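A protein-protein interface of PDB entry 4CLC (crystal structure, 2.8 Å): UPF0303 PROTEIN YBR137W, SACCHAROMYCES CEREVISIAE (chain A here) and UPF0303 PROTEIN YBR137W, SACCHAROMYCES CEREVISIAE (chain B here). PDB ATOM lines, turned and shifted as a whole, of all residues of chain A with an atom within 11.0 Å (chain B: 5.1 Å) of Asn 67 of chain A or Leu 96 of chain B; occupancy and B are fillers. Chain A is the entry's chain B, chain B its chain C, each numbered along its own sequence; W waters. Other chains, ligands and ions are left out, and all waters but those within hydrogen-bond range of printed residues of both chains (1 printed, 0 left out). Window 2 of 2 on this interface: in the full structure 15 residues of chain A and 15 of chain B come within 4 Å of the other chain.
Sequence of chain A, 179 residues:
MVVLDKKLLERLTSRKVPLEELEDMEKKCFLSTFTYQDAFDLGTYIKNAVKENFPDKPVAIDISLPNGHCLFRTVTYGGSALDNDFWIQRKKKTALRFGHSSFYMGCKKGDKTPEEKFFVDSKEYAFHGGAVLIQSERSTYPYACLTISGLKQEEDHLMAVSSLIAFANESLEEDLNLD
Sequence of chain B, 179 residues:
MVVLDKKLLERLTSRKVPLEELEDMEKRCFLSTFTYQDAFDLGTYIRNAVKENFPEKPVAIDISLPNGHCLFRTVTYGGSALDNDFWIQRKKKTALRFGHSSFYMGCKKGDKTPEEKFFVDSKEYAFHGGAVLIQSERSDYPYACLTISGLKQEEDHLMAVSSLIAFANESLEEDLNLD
Asn 67 of chain A touches just these residues of chain B: Pro 66 and Leu 96.
No residue of chain A comes within 4 Å of Lys 92 of chain B.
No residue of chain A comes within 4 Å of Ala 95 of chain B.
No residue of chain A comes within 4 Å of Cys 145 of chain B.
Of the printed residues of chain B, Pro 66 of chain A touches Asn 67 (3.1 Å).
Of the printed residues of chain A, Pro 66 of chain B touches Asn 67 (3.1 Å).
Printed residues of chain A within 4 Å of Leu 65 of chain B: Tyr 141.
Lys 93 of chain A touches none of the printed residues of chain B.
Leu 65 of chain A touches none of the printed residues of chain B.
The nearest printed residue of chain B that does not touch Leu 96 of chain A is Leu 65 of chain B (7.1 Å).
N of His 69 of chain A lies close to OD1 of Asn 67 of chain A (3.4 Å).
Among the printed residues, merely in contact across the chains: Asn 67 of chain A with Pro 66 of chain B (3.1 Å), Pro 66 of chain A with Asn 67 of chain B (3.1 Å) and Tyr 141 of chain A with Leu 65 of chain B (3.8 Å).
Of the 14 printed residues of chain B, 4 touch a printed residue of chain A.
Along chain B the printed residues that touch a printed residue of chain A span positions 65 to 96.
Among the printed residues, 5 pairs touch across the chains.
The backbone carbonyl oxygen (O) of Leu 96 of chain B is in hydrogen-bond range of the side-chain amide nitrogen (ND2) of Asn 67 of chain A (3.4 Å).
The backbone carbonyl oxygen (O) of Leu 96 of chain A is in hydrogen-bond range of the side-chain amide nitrogen (ND2) of Asn 67 of chain B (3.3 Å).
Water W1 lies within hydrogen-bond range of ND2 of Asn 67 of chain B, O of Leu 96 of chain A and O of Arg 97 of chain A.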
ATOM      1  N   PHE A  34      26.034   1.284  -5.958  1.00  0.00           N
ATOM      2  CA  PHE A  34      24.636   0.962  -5.699  1.00  0.00           C
ATOM      3  C   PHE A  34      24.148   1.587  -4.397  1.00  0.00           C
ATOM      4  O   PHE A  34      24.614   1.220  -3.332  1.00  0.00           O
ATOM      5  CB  PHE A  34      24.438  -0.553  -5.660  1.00  0.00           C
ATOM      6  CG  PHE A  34      23.019  -0.976  -5.859  1.00  0.00           C
ATOM      7  CD1 PHE A  34      22.375  -0.732  -7.062  1.00  0.00           C
ATOM      8  CD2 PHE A  34      22.320  -1.614  -4.845  1.00  0.00           C
ATOM      9  CE1 PHE A  34      21.052  -1.119  -7.255  1.00  0.00           C
ATOM     10  CE2 PHE A  34      21.005  -2.008  -5.028  1.00  0.00           C
ATOM     11  CZ  PHE A  34      20.367  -1.758  -6.234  1.00  0.00           C
ATOM     12  N   ASP A  62      10.218  -4.118  -9.914  1.00  0.00           N
ATOM     13  CA  ASP A  62      10.706  -4.337  -8.569  1.00  0.00           C
ATOM     14  C   ASP A  62      12.223  -4.461  -8.568  1.00  0.00           C
ATOM     15  O   ASP A  62      12.786  -5.135  -9.431  1.00  0.00           O
ATOM     16  CB  ASP A  62      10.068  -5.603  -7.987  1.00  0.00           C
ATOM     17  CG  ASP A  62      10.503  -5.878  -6.561  1.00  0.00           C
ATOM     18  OD1 ASP A  62       9.828  -5.355  -5.643  1.00  0.00           O
ATOM     19  OD2 ASP A  62      11.509  -6.613  -6.360  1.00  0.00           O
ATOM     20  N   ILE A  63      12.878  -3.796  -7.615  1.00  0.00           N
ATOM     21  CA  ILE A  63      14.275  -4.082  -7.302  1.00  0.00           C
ATOM     22  C   ILE A  63      14.382  -4.465  -5.850  1.00  0.00           C
ATOM     23  O   ILE A  63      14.056  -3.654  -4.982  1.00  0.00           O
ATOM     24  CB  ILE A  63      15.221  -2.882  -7.500  1.00  0.00           C
ATOM     25  CG1 ILE A  63      15.025  -2.203  -8.844  1.00  0.00           C
ATOM     26  CG2 ILE A  63      16.673  -3.326  -7.338  1.00  0.00           C
ATOM     27  CD1 ILE A  63      15.762  -0.915  -8.914  1.00  0.00           C
ATOM     28  N   SER A  64      14.850  -5.677  -5.569  1.00  0.00           N
ATOM     29  CA  SER A  64      15.057  -6.100  -4.184  1.00  0.00           C
ATOM     30  C   SER A  64      16.480  -6.626  -4.037  1.00  0.00           C
ATOM     31  O   SER A  64      17.195  -6.740  -5.021  1.00  0.00           O
ATOM     32  CB  SER A  64      14.042  -7.166  -3.781  1.00  0.00           C
ATOM     33  OG  SER A  64      12.705  -6.726  -3.974  1.00  0.00           O
ATOM     34  N   LEU A  65      16.865  -7.018  -2.833  1.00  0.00           N
ATOM     35  CA  LEU A  65      18.246  -7.394  -2.559  1.00  0.00           C
ATOM     36  C   LEU A  65      18.298  -8.900  -2.337  1.00  0.00           C
ATOM     37  O   LEU A  65      17.277  -9.512  -2.029  1.00  0.00           O
ATOM     38  CB  LEU A  65      18.784  -6.663  -1.321  1.00  0.00           C
ATOM     39  CG  LEU A  65      18.813  -5.143  -1.205  1.00  0.00           C
ATOM     40  CD1 LEU A  65      19.347  -4.792   0.164  1.00  0.00           C
ATOM     41  CD2 LEU A  65      19.660  -4.515  -2.287  1.00  0.00           C
ATOM     42  N   PRO A  66      19.479  -9.515  -2.496  1.00  0.00           N
ATOM     43  CA  PRO A  66      19.553 -10.982  -2.422  1.00  0.00           C
ATOM     44  C   PRO A  66      18.846 -11.596  -1.204  1.00  0.00           C
ATOM     45  O   PRO A  66      18.452 -12.771  -1.250  1.00  0.00           O
ATOM     46  CB  PRO A  66      21.063 -11.243  -2.355  1.00  0.00           C
ATOM     47  CG  PRO A  66      21.660 -10.086  -3.118  1.00  0.00           C
ATOM     48  CD  PRO A  66      20.788  -8.907  -2.795  1.00  0.00           C
ATOM     49  N   ASN A  67      18.677 -10.812  -0.141  1.00  0.00           N
ATOM     50  CA  ASN A  67      18.051 -11.310   1.068  1.00  0.00           C
ATOM     51  C   ASN A  67      16.545 -11.000   1.079  1.00  0.00           C
ATOM     52  O   ASN A  67      15.832 -11.328   2.029  1.00  0.00           O
ATOM     53  CB  ASN A  67      18.746 -10.737   2.300  1.00  0.00           C
ATOM     54  CG  ASN A  67      18.368  -9.294   2.573  1.00  0.00           C
ATOM     55  OD1 ASN A  67      18.214  -8.497   1.655  1.00  0.00           O
ATOM     56  ND2 ASN A  67      18.220  -8.952   3.846  1.00  0.00           N
ATOM     57  N   GLY A  68      16.057 -10.396   0.005  1.00  0.00           N
ATOM     58  CA  GLY A  68      14.632 -10.219  -0.157  1.00  0.00           C
ATOM     59  C   GLY A  68      14.115  -8.858   0.244  1.00  0.00           C
ATOM     60  O   GLY A  68      12.937  -8.552   0.037  1.00  0.00           O
ATOM     61  N   HIS A  69      14.984  -8.033   0.818  1.00  0.00           N
ATOM     62  CA  HIS A  69      14.596  -6.678   1.195  1.00  0.00           C
ATOM     63  C   HIS A  69      14.214  -5.874  -0.031  1.00  0.00           C
ATOM     64  O   HIS A  69      15.003  -5.759  -0.971  1.00  0.00           O
ATOM     65  CB  HIS A  69      15.738  -6.000   1.953  1.00  0.00           C
ATOM     66  CG  HIS A  69      15.461  -4.571   2.317  1.00  0.00           C
ATOM     67  ND1 HIS A  69      14.202  -4.110   2.621  1.00  0.00           N
ATOM     68  CD2 HIS A  69      16.294  -3.501   2.433  1.00  0.00           C
ATOM     69  CE1 HIS A  69      14.260  -2.819   2.900  1.00  0.00           C
ATOM     70  NE2 HIS A  69      15.513  -2.426   2.800  1.00  0.00           N
ATOM     71  N   CYS A  70      13.009  -5.307  -0.018  1.00  0.00           N
ATOM     72  CA  CYS A  70      12.480  -4.636  -1.209  1.00  0.00           C
ATOM     73  C   CYS A  70      12.700  -3.131  -1.216  1.00  0.00           C
ATOM     74  O   CYS A  70      12.085  -2.416  -0.439  1.00  0.00           O
ATOM     75  CB  CYS A  70      10.992  -4.906  -1.346  1.00  0.00           C
ATOM     76  SG  CYS A  70      10.292  -4.040  -2.716  1.00  0.00           S
ATOM     77  N   LEU A  71      13.572  -2.667  -2.110  1.00  0.00           N
ATOM     78  CA  LEU A  71      13.951  -1.262  -2.195  1.00  0.00           C
ATOM     79  C   LEU A  71      12.968  -0.412  -2.997  1.00  0.00           C
ATOM     80  O   LEU A  71      12.746   0.759  -2.680  1.00  0.00           O
ATOM     81  CB  LEU A  71      15.347  -1.130  -2.802  1.00  0.00           C
ATOM     82  CG  LEU A  71      16.473  -1.744  -1.969  1.00  0.00           C
ATOM     83  CD1 LEU A  71      17.858  -1.281  -2.435  1.00  0.00           C
ATOM     84  CD2 LEU A  71      16.261  -1.492  -0.475  1.00  0.00           C
ATOM     85  N   GLN A  89       7.921 -12.309  -7.348  1.00  0.00           N
ATOM     86  CA  GLN A  89       8.494 -13.148  -6.318  1.00  0.00           C
ATOM     87  C   GLN A  89       9.134 -14.372  -6.965  1.00  0.00           C
ATOM     88  O   GLN A  89      10.328 -14.658  -6.774  1.00  0.00           O
ATOM     89  CB  GLN A  89       7.416 -13.547  -5.314  1.00  0.00           C
ATOM     90  CG  GLN A  89       7.950 -14.085  -3.988  1.00  0.00           C
ATOM     91  CD  GLN A  89       8.785 -13.062  -3.253  1.00  0.00           C
ATOM     92  OE1 GLN A  89       8.765 -11.863  -3.580  1.00  0.00           O
ATOM     93  NE2 GLN A  89       9.547 -13.525  -2.262  1.00  0.00           N
ATOM     94  N   LYS A  92      12.083 -13.755  -9.454  1.00  0.00           N
ATOM     95  CA  LYS A  92      13.197 -13.219  -8.669  1.00  0.00           C
ATOM     96  C   LYS A  92      13.936 -14.342  -7.961  1.00  0.00           C
ATOM     97  O   LYS A  92      15.159 -14.402  -7.989  1.00  0.00           O
ATOM     98  CB  LYS A  92      12.712 -12.184  -7.647  1.00  0.00           C
ATOM     99  CG  LYS A  92      13.824 -11.546  -6.794  1.00  0.00           C
ATOM    100  CD  LYS A  92      13.256 -10.692  -5.647  1.00  0.00           C
ATOM    101  CE  LYS A  92      12.286 -11.491  -4.768  1.00  0.00           C
ATOM    102  NZ  LYS A  92      11.666 -10.669  -3.684  1.00  0.00           N
ATOM    103  N   LYS A  93      13.180 -15.248  -7.355  1.00  0.00           N
ATOM    104  CA  LYS A  93      13.763 -16.337  -6.589  1.00  0.00           C
ATOM    105  C   LYS A  93      14.646 -17.207  -7.468  1.00  0.00           C
ATOM    106  O   LYS A  93      15.722 -17.633  -7.059  1.00  0.00           O
ATOM    107  CB  LYS A  93      12.657 -17.165  -5.940  1.00  0.00           C
ATOM    108  CG  LYS A  93      13.110 -17.992  -4.741  1.00  0.00           C
ATOM    109  CD  LYS A  93      11.914 -18.477  -3.942  1.00  0.00           C
ATOM    110  CE  LYS A  93      12.341 -19.179  -2.679  1.00  0.00           C
ATOM    111  NZ  LYS A  93      11.136 -19.574  -1.904  1.00  0.00           N
ATOM    112  N   ALA A  95      16.121 -16.196 -10.387  1.00  0.00           N
ATOM    113  CA  ALA A  95      17.276 -15.399 -10.748  1.00  0.00           C
ATOM    114  C   ALA A  95      18.257 -15.305  -9.580  1.00  0.00           C
ATOM    115  O   ALA A  95      19.463 -15.431  -9.769  1.00  0.00           O
ATOM    116  CB  ALA A  95      16.840 -14.021 -11.205  1.00  0.00           C
ATOM    117  N   LEU A  96      17.733 -15.116  -8.371  1.00  0.00           N
ATOM    118  CA  LEU A  96      18.586 -15.022  -7.180  1.00  0.00           C
ATOM    119  C   LEU A  96      19.225 -16.345  -6.814  1.00  0.00           C
ATOM    120  O   LEU A  96      20.379 -16.373  -6.374  1.00  0.00           O
ATOM    121  CB  LEU A  96      17.802 -14.496  -5.990  1.00  0.00           C
ATOM    122  CG  LEU A  96      17.865 -12.983  -6.030  1.00  0.00           C
ATOM    123  CD1 LEU A  96      16.941 -12.393  -5.017  1.00  0.00           C
ATOM    124  CD2 LEU A  96      19.297 -12.579  -5.775  1.00  0.00           C
ATOM    125  N   ARG A  97      18.488 -17.439  -7.011  1.00  0.00           N
ATOM    126  CA  ARG A  97      18.987 -18.752  -6.624  1.00  0.00           C
ATOM    127  C   ARG A  97      20.018 -19.323  -7.594  1.00  0.00           C
ATOM    128  O   ARG A  97      21.041 -19.827  -7.163  1.00  0.00           O
ATOM    129  CB  ARG A  97      17.844 -19.745  -6.469  1.00  0.00           C
ATOM    130  CG  ARG A  97      18.373 -21.124  -6.221  1.00  0.00           C
ATOM    131  CD  ARG A  97      17.301 -22.124  -5.952  1.00  0.00           C
ATOM    132  NE  ARG A  97      17.880 -23.446  -6.084  1.00  0.00           N
ATOM    133  CZ  ARG A  97      17.329 -24.558  -5.632  1.00  0.00           C
ATOM    134  NH1 ARG A  97      16.172 -24.514  -4.984  1.00  0.00           N
ATOM    135  NH2 ARG A  97      17.962 -25.710  -5.814  1.00  0.00           N
ATOM    136  N   LEU A 133      19.672 -10.058 -12.747  1.00  0.00           N
ATOM    137  CA  LEU A 133      20.553  -9.661 -11.662  1.00  0.00           C
ATOM    138  C   LEU A 133      21.349  -8.389 -11.960  1.00  0.00           C
ATOM    139  O   LEU A 133      22.078  -8.335 -12.951  1.00  0.00           O
ATOM    140  CB  LEU A 133      21.530 -10.796 -11.353  1.00  0.00           C
ATOM    141  CG  LEU A 133      20.954 -12.152 -10.932  1.00  0.00           C
ATOM    142  CD1 LEU A 133      22.071 -13.176 -10.831  1.00  0.00           C
ATOM    143  CD2 LEU A 133      20.156 -12.073  -9.623  1.00  0.00           C
ATOM    144  N   TYR A 141      29.648 -11.413  -7.124  1.00  0.00           N
ATOM    145  CA  TYR A 141      28.257 -11.673  -6.724  1.00  0.00           C
ATOM    146  C   TYR A 141      27.430 -10.381  -6.874  1.00  0.00           C
ATOM    147  O   TYR A 141      28.000  -9.282  -6.861  1.00  0.00           O
ATOM    148  CB  TYR A 141      28.233 -12.231  -5.302  1.00  0.00           C
ATOM    149  CG  TYR A 141      29.275 -13.305  -5.120  1.00  0.00           C
ATOM    150  CD1 TYR A 141      29.047 -14.609  -5.558  1.00  0.00           C
ATOM    151  CD2 TYR A 141      30.514 -13.011  -4.567  1.00  0.00           C
ATOM    152  CE1 TYR A 141      30.005 -15.583  -5.424  1.00  0.00           C
ATOM    153  CE2 TYR A 141      31.477 -13.988  -4.424  1.00  0.00           C
ATOM    154  CZ  TYR A 141      31.217 -15.261  -4.863  1.00  0.00           C
ATOM    155  OH  TYR A 141      32.176 -16.216  -4.725  1.00  0.00           O
ATOM    156  N   PRO A 142      26.100 -10.505  -7.087  1.00  0.00           N
ATOM    157  CA  PRO A 142      25.255  -9.370  -7.480  1.00  0.00           C
ATOM    158  C   PRO A 142      24.769  -8.460  -6.349  1.00  0.00           C
ATOM    159  O   PRO A 142      24.532  -8.913  -5.230  1.00  0.00           O
ATOM    160  CB  PRO A 142      24.069 -10.057  -8.150  1.00  0.00           C
ATOM    161  CG  PRO A 142      23.932 -11.316  -7.405  1.00  0.00           C
ATOM    162  CD  PRO A 142      25.311 -11.739  -6.964  1.00  0.00           C
ATOM    163  N   TYR A 143      24.570  -7.190  -6.680  1.00  0.00           N
ATOM    164  CA  TYR A 143      24.041  -6.193  -5.746  1.00  0.00           C
ATOM    165  C   TYR A 143      22.642  -6.541  -5.331  1.00  0.00           C
ATOM    166  O   TYR A 143      22.334  -6.656  -4.152  1.00  0.00           O
ATOM    167  CB  TYR A 143      24.010  -4.792  -6.383  1.00  0.00           C
ATOM    168  CG  TYR A 143      25.321  -4.055  -6.367  1.00  0.00           C
ATOM    169  CD1 TYR A 143      26.233  -4.253  -5.332  1.00  0.00           C
ATOM    170  CD2 TYR A 143      25.654  -3.166  -7.383  1.00  0.00           C
ATOM    171  CE1 TYR A 143      27.434  -3.579  -5.296  1.00  0.00           C
ATOM    172  CE2 TYR A 143      26.854  -2.481  -7.359  1.00  0.00           C
ATOM    173  CZ  TYR A 143      27.745  -2.693  -6.309  1.00  0.00           C
ATOM    174  OH  TYR A 143      28.959  -2.032  -6.260  1.00  0.00           O
ATOM    175  N   ALA A 144      21.796  -6.689  -6.340  1.00  0.00           N
ATOM    176  CA  ALA A 144      20.363  -6.790  -6.161  1.00  0.00           C
ATOM    177  C   ALA A 144      19.761  -7.536  -7.328  1.00  0.00           C
ATOM    178  O   ALA A 144      20.476  -8.114  -8.146  1.00  0.00           O
ATOM    179  CB  ALA A 144      19.762  -5.428  -6.045  1.00  0.00           C
ATOM    180  N   CYS A 145      18.441  -7.528  -7.402  1.00  0.00           N
ATOM    181  CA  CYS A 145      17.754  -8.146  -8.522  1.00  0.00           C
ATOM    182  C   CYS A 145      16.693  -7.205  -9.075  1.00  0.00           C
ATOM    183  O   CYS A 145      15.932  -6.579  -8.320  1.00  0.00           O
ATOM    184  CB  CYS A 145      17.126  -9.487  -8.106  1.00  0.00           C
ATOM    185  SG  CYS A 145      16.249 -10.392  -9.446  1.00  0.00           S
ATOM    186  N   LEU B  65      26.556 -15.216   1.547  1.00  0.00           N
ATOM    187  CA  LEU B  65      25.887 -14.076   0.940  1.00  0.00           C
ATOM    188  C   LEU B  65      24.555 -13.826   1.642  1.00  0.00           C
ATOM    189  O   LEU B  65      24.051 -14.687   2.354  1.00  0.00           O
ATOM    190  CB  LEU B  65      25.656 -14.306  -0.558  1.00  0.00           C
ATOM    191  CG  LEU B  65      26.796 -14.742  -1.474  1.00  0.00           C
ATOM    192  CD1 LEU B  65      26.280 -14.718  -2.889  1.00  0.00           C
ATOM    193  CD2 LEU B  65      28.019 -13.864  -1.323  1.00  0.00           C
ATOM    194  N   PRO B  66      23.980 -12.640   1.434  1.00  0.00           N
ATOM    195  CA  PRO B  66      22.668 -12.341   2.003  1.00  0.00           C
ATOM    196  C   PRO B  66      21.558 -13.251   1.525  1.00  0.00           C
ATOM    197  O   PRO B  66      20.511 -13.259   2.160  1.00  0.00           O
ATOM    198  CB  PRO B  66      22.408 -10.912   1.537  1.00  0.00           C
ATOM    199  CG  PRO B  66      23.767 -10.331   1.348  1.00  0.00           C
ATOM    200  CD  PRO B  66      24.585 -11.455   0.800  1.00  0.00           C
ATOM    201  N   ASN B  67      21.743 -13.988   0.434  1.00  0.00           N
ATOM    202  CA  ASN B  67      20.710 -14.935   0.014  1.00  0.00           C
ATOM    203  C   ASN B  67      20.945 -16.335   0.596  1.00  0.00           C
ATOM    204  O   ASN B  67      20.126 -17.246   0.418  1.00  0.00           O
ATOM    205  CB  ASN B  67      20.631 -14.999  -1.509  1.00  0.00           C
ATOM    206  CG  ASN B  67      21.804 -15.734  -2.130  1.00  0.00           C
ATOM    207  OD1 ASN B  67      22.887 -15.847  -1.548  1.00  0.00           O
ATOM    208  ND2 ASN B  67      21.588 -16.238  -3.330  1.00  0.00           N
ATOM    209  N   LYS B  92      23.444 -15.159  12.069  1.00  0.00           N
ATOM    210  CA  LYS B  92      23.529 -14.659  10.700  1.00  0.00           C
ATOM    211  C   LYS B  92      22.188 -14.110  10.241  1.00  0.00           C
ATOM    212  O   LYS B  92      22.116 -13.081   9.567  1.00  0.00           O
ATOM    213  CB  LYS B  92      24.016 -15.771   9.769  1.00  0.00           C
ATOM    214  CG  LYS B  92      24.238 -15.385   8.332  1.00  0.00           C
ATOM    215  CD  LYS B  92      24.968 -16.508   7.551  1.00  0.00           C
ATOM    216  CE  LYS B  92      24.140 -17.805   7.432  1.00  0.00           C
ATOM    217  NZ  LYS B  92      22.861 -17.584   6.684  1.00  0.00           N
ATOM    218  N   LYS B  93      21.127 -14.795  10.633  1.00  0.00           N
ATOM    219  CA  LYS B  93      19.806 -14.392  10.251  1.00  0.00           C
ATOM    220  C   LYS B  93      19.479 -13.008  10.839  1.00  0.00           C
ATOM    221  O   LYS B  93      18.980 -12.126  10.128  1.00  0.00           O
ATOM    222  CB  LYS B  93      18.805 -15.466  10.690  1.00  0.00           C
ATOM    223  CG  LYS B  93      17.406 -15.239  10.161  1.00  0.00           C
ATOM    224  CD  LYS B  93      16.610 -16.510  10.093  1.00  0.00           C
ATOM    225  CE  LYS B  93      15.519 -16.374   9.045  1.00  0.00           C
ATOM    226  NZ  LYS B  93      14.795 -17.662   8.855  1.00  0.00           N
ATOM    227  N   THR B  94      19.782 -12.815  12.127  1.00  0.00           N
ATOM    228  CA  THR B  94      19.661 -11.508  12.783  1.00  0.00           C
ATOM    229  C   THR B  94      20.429 -10.401  12.044  1.00  0.00           C
ATOM    230  O   THR B  94      19.864  -9.383  11.657  1.00  0.00           O
ATOM    231  CB  THR B  94      20.203 -11.545  14.248  1.00  0.00           C
ATOM    232  OG1 THR B  94      19.403 -12.395  15.077  1.00  0.00           O
ATOM    233  CG2 THR B  94      20.253 -10.135  14.847  1.00  0.00           C
ATOM    234  N   ALA B  95      21.730 -10.602  11.868  1.00  0.00           N
ATOM    235  CA  ALA B  95      22.572  -9.610  11.212  1.00  0.00           C
ATOM    236  C   ALA B  95      22.041  -9.229   9.838  1.00  0.00           C
ATOM    237  O   ALA B  95      22.004  -8.053   9.491  1.00  0.00           O
ATOM    238  CB  ALA B  95      24.001 -10.127  11.095  1.00  0.00           C
ATOM    239  N   LEU B  96      21.633 -10.223   9.055  1.00  0.00           N
ATOM    240  CA  LEU B  96      21.215  -9.960   7.688  1.00  0.00           C
ATOM    241  C   LEU B  96      19.882  -9.251   7.685  1.00  0.00           C
ATOM    242  O   LEU B  96      19.657  -8.350   6.881  1.00  0.00           O
ATOM    243  CB  LEU B  96      21.156 -11.259   6.864  1.00  0.00           C
ATOM    244  CG  LEU B  96      22.484 -11.734   6.254  1.00  0.00           C
ATOM    245  CD1 LEU B  96      22.394 -13.120   5.689  1.00  0.00           C
ATOM    246  CD2 LEU B  96      22.921 -10.770   5.187  1.00  0.00           C
ATOM    247  N   ARG B  97      19.015  -9.638   8.609  1.00  0.00           N
ATOM    248  CA  ARG B  97      17.683  -9.048   8.699  1.00  0.00           C
ATOM    249  C   ARG B  97      17.665  -7.592   9.190  1.00  0.00           C
ATOM    250  O   ARG B  97      16.954  -6.748   8.628  1.00  0.00           O
ATOM    251  CB  ARG B  97      16.786  -9.884   9.619  1.00  0.00           C
ATOM    252  CG  ARG B  97      15.417  -9.253   9.829  1.00  0.00           C
ATOM    253  CD  ARG B  97      14.531 -10.141  10.633  1.00  0.00           C
ATOM    254  NE  ARG B  97      13.335  -9.436  11.075  1.00  0.00           N
ATOM    255  CZ  ARG B  97      12.152 -10.010  11.250  1.00  0.00           C
ATOM    256  NH1 ARG B  97      11.992 -11.304  10.997  1.00  0.00           N
ATOM    257  NH2 ARG B  97      11.133  -9.285  11.665  1.00  0.00           N
ATOM    258  N   PHE B  98      18.407  -7.309  10.256  1.00  0.00           N
ATOM    259  CA  PHE B  98      18.339  -5.995  10.858  1.00  0.00           C
ATOM    260  C   PHE B  98      19.386  -4.984  10.360  1.00  0.00           C
ATOM    261  O   PHE B  98      19.250  -3.781  10.604  1.00  0.00           O
ATOM    262  CB  PHE B  98      18.448  -6.138  12.373  1.00  0.00           C
ATOM    263  CG  PHE B  98      17.300  -6.878  13.002  1.00  0.00           C
ATOM    264  CD1 PHE B  98      16.108  -6.221  13.282  1.00  0.00           C
ATOM    265  CD2 PHE B  98      17.415  -8.232  13.319  1.00  0.00           C
ATOM    266  CE1 PHE B  98      15.052  -6.899  13.850  1.00  0.00           C
ATOM    267  CE2 PHE B  98      16.360  -8.917  13.890  1.00  0.00           C
ATOM    268  CZ  PHE B  98      15.175  -8.245  14.162  1.00  0.00           C
ATOM    269  N   GLY B  99      20.400  -5.443   9.638  1.00  0.00           N
ATOM    270  CA  GLY B  99      21.445  -4.544   9.188  1.00  0.00           C
ATOM    271  C   GLY B  99      22.425  -4.034  10.249  1.00  0.00           C
ATOM    272  O   GLY B  99      23.029  -2.966  10.089  1.00  0.00           O
ATOM    273  N   LEU B 133      28.264  -8.025   9.460  1.00  0.00           N
ATOM    274  CA  LEU B 133      28.090  -7.897   8.021  1.00  0.00           C
ATOM    275  C   LEU B 133      29.393  -7.500   7.327  1.00  0.00           C
ATOM    276  O   LEU B 133      30.192  -6.757   7.886  1.00  0.00           O
ATOM    277  CB  LEU B 133      26.990  -6.876   7.713  1.00  0.00           C
ATOM    278  CG  LEU B 133      25.600  -7.240   8.250  1.00  0.00           C
ATOM    279  CD1 LEU B 133      24.565  -6.154   7.992  1.00  0.00           C
ATOM    280  CD2 LEU B 133      25.152  -8.572   7.656  1.00  0.00           C
ATOM    281  N   ALA B 144      28.200  -9.520   2.094  1.00  0.00           N
ATOM    282  CA  ALA B 144      28.003 -10.826   2.696  1.00  0.00           C
ATOM    283  C   ALA B 144      27.839 -10.675   4.201  1.00  0.00           C
ATOM    284  O   ALA B 144      27.642  -9.563   4.692  1.00  0.00           O
ATOM    285  CB  ALA B 144      29.166 -11.737   2.372  1.00  0.00           C
ATOM    286  N   CYS B 145      27.874 -11.796   4.919  1.00  0.00           N
ATOM    287  CA  CYS B 145      27.923 -11.767   6.373  1.00  0.00           C
ATOM    288  C   CYS B 145      29.055 -12.650   6.868  1.00  0.00           C
ATOM    289  O   CYS B 145      29.276 -13.730   6.354  1.00  0.00           O
ATOM    290  CB  CYS B 145      26.588 -12.215   6.983  1.00  0.00           C
ATOM    291  SG  CYS B 145      26.537 -12.241   8.825  1.00  0.00           S
HETATM  292  O   HOH W   1      22.738 -17.620  -5.326  1.00  0.00           O
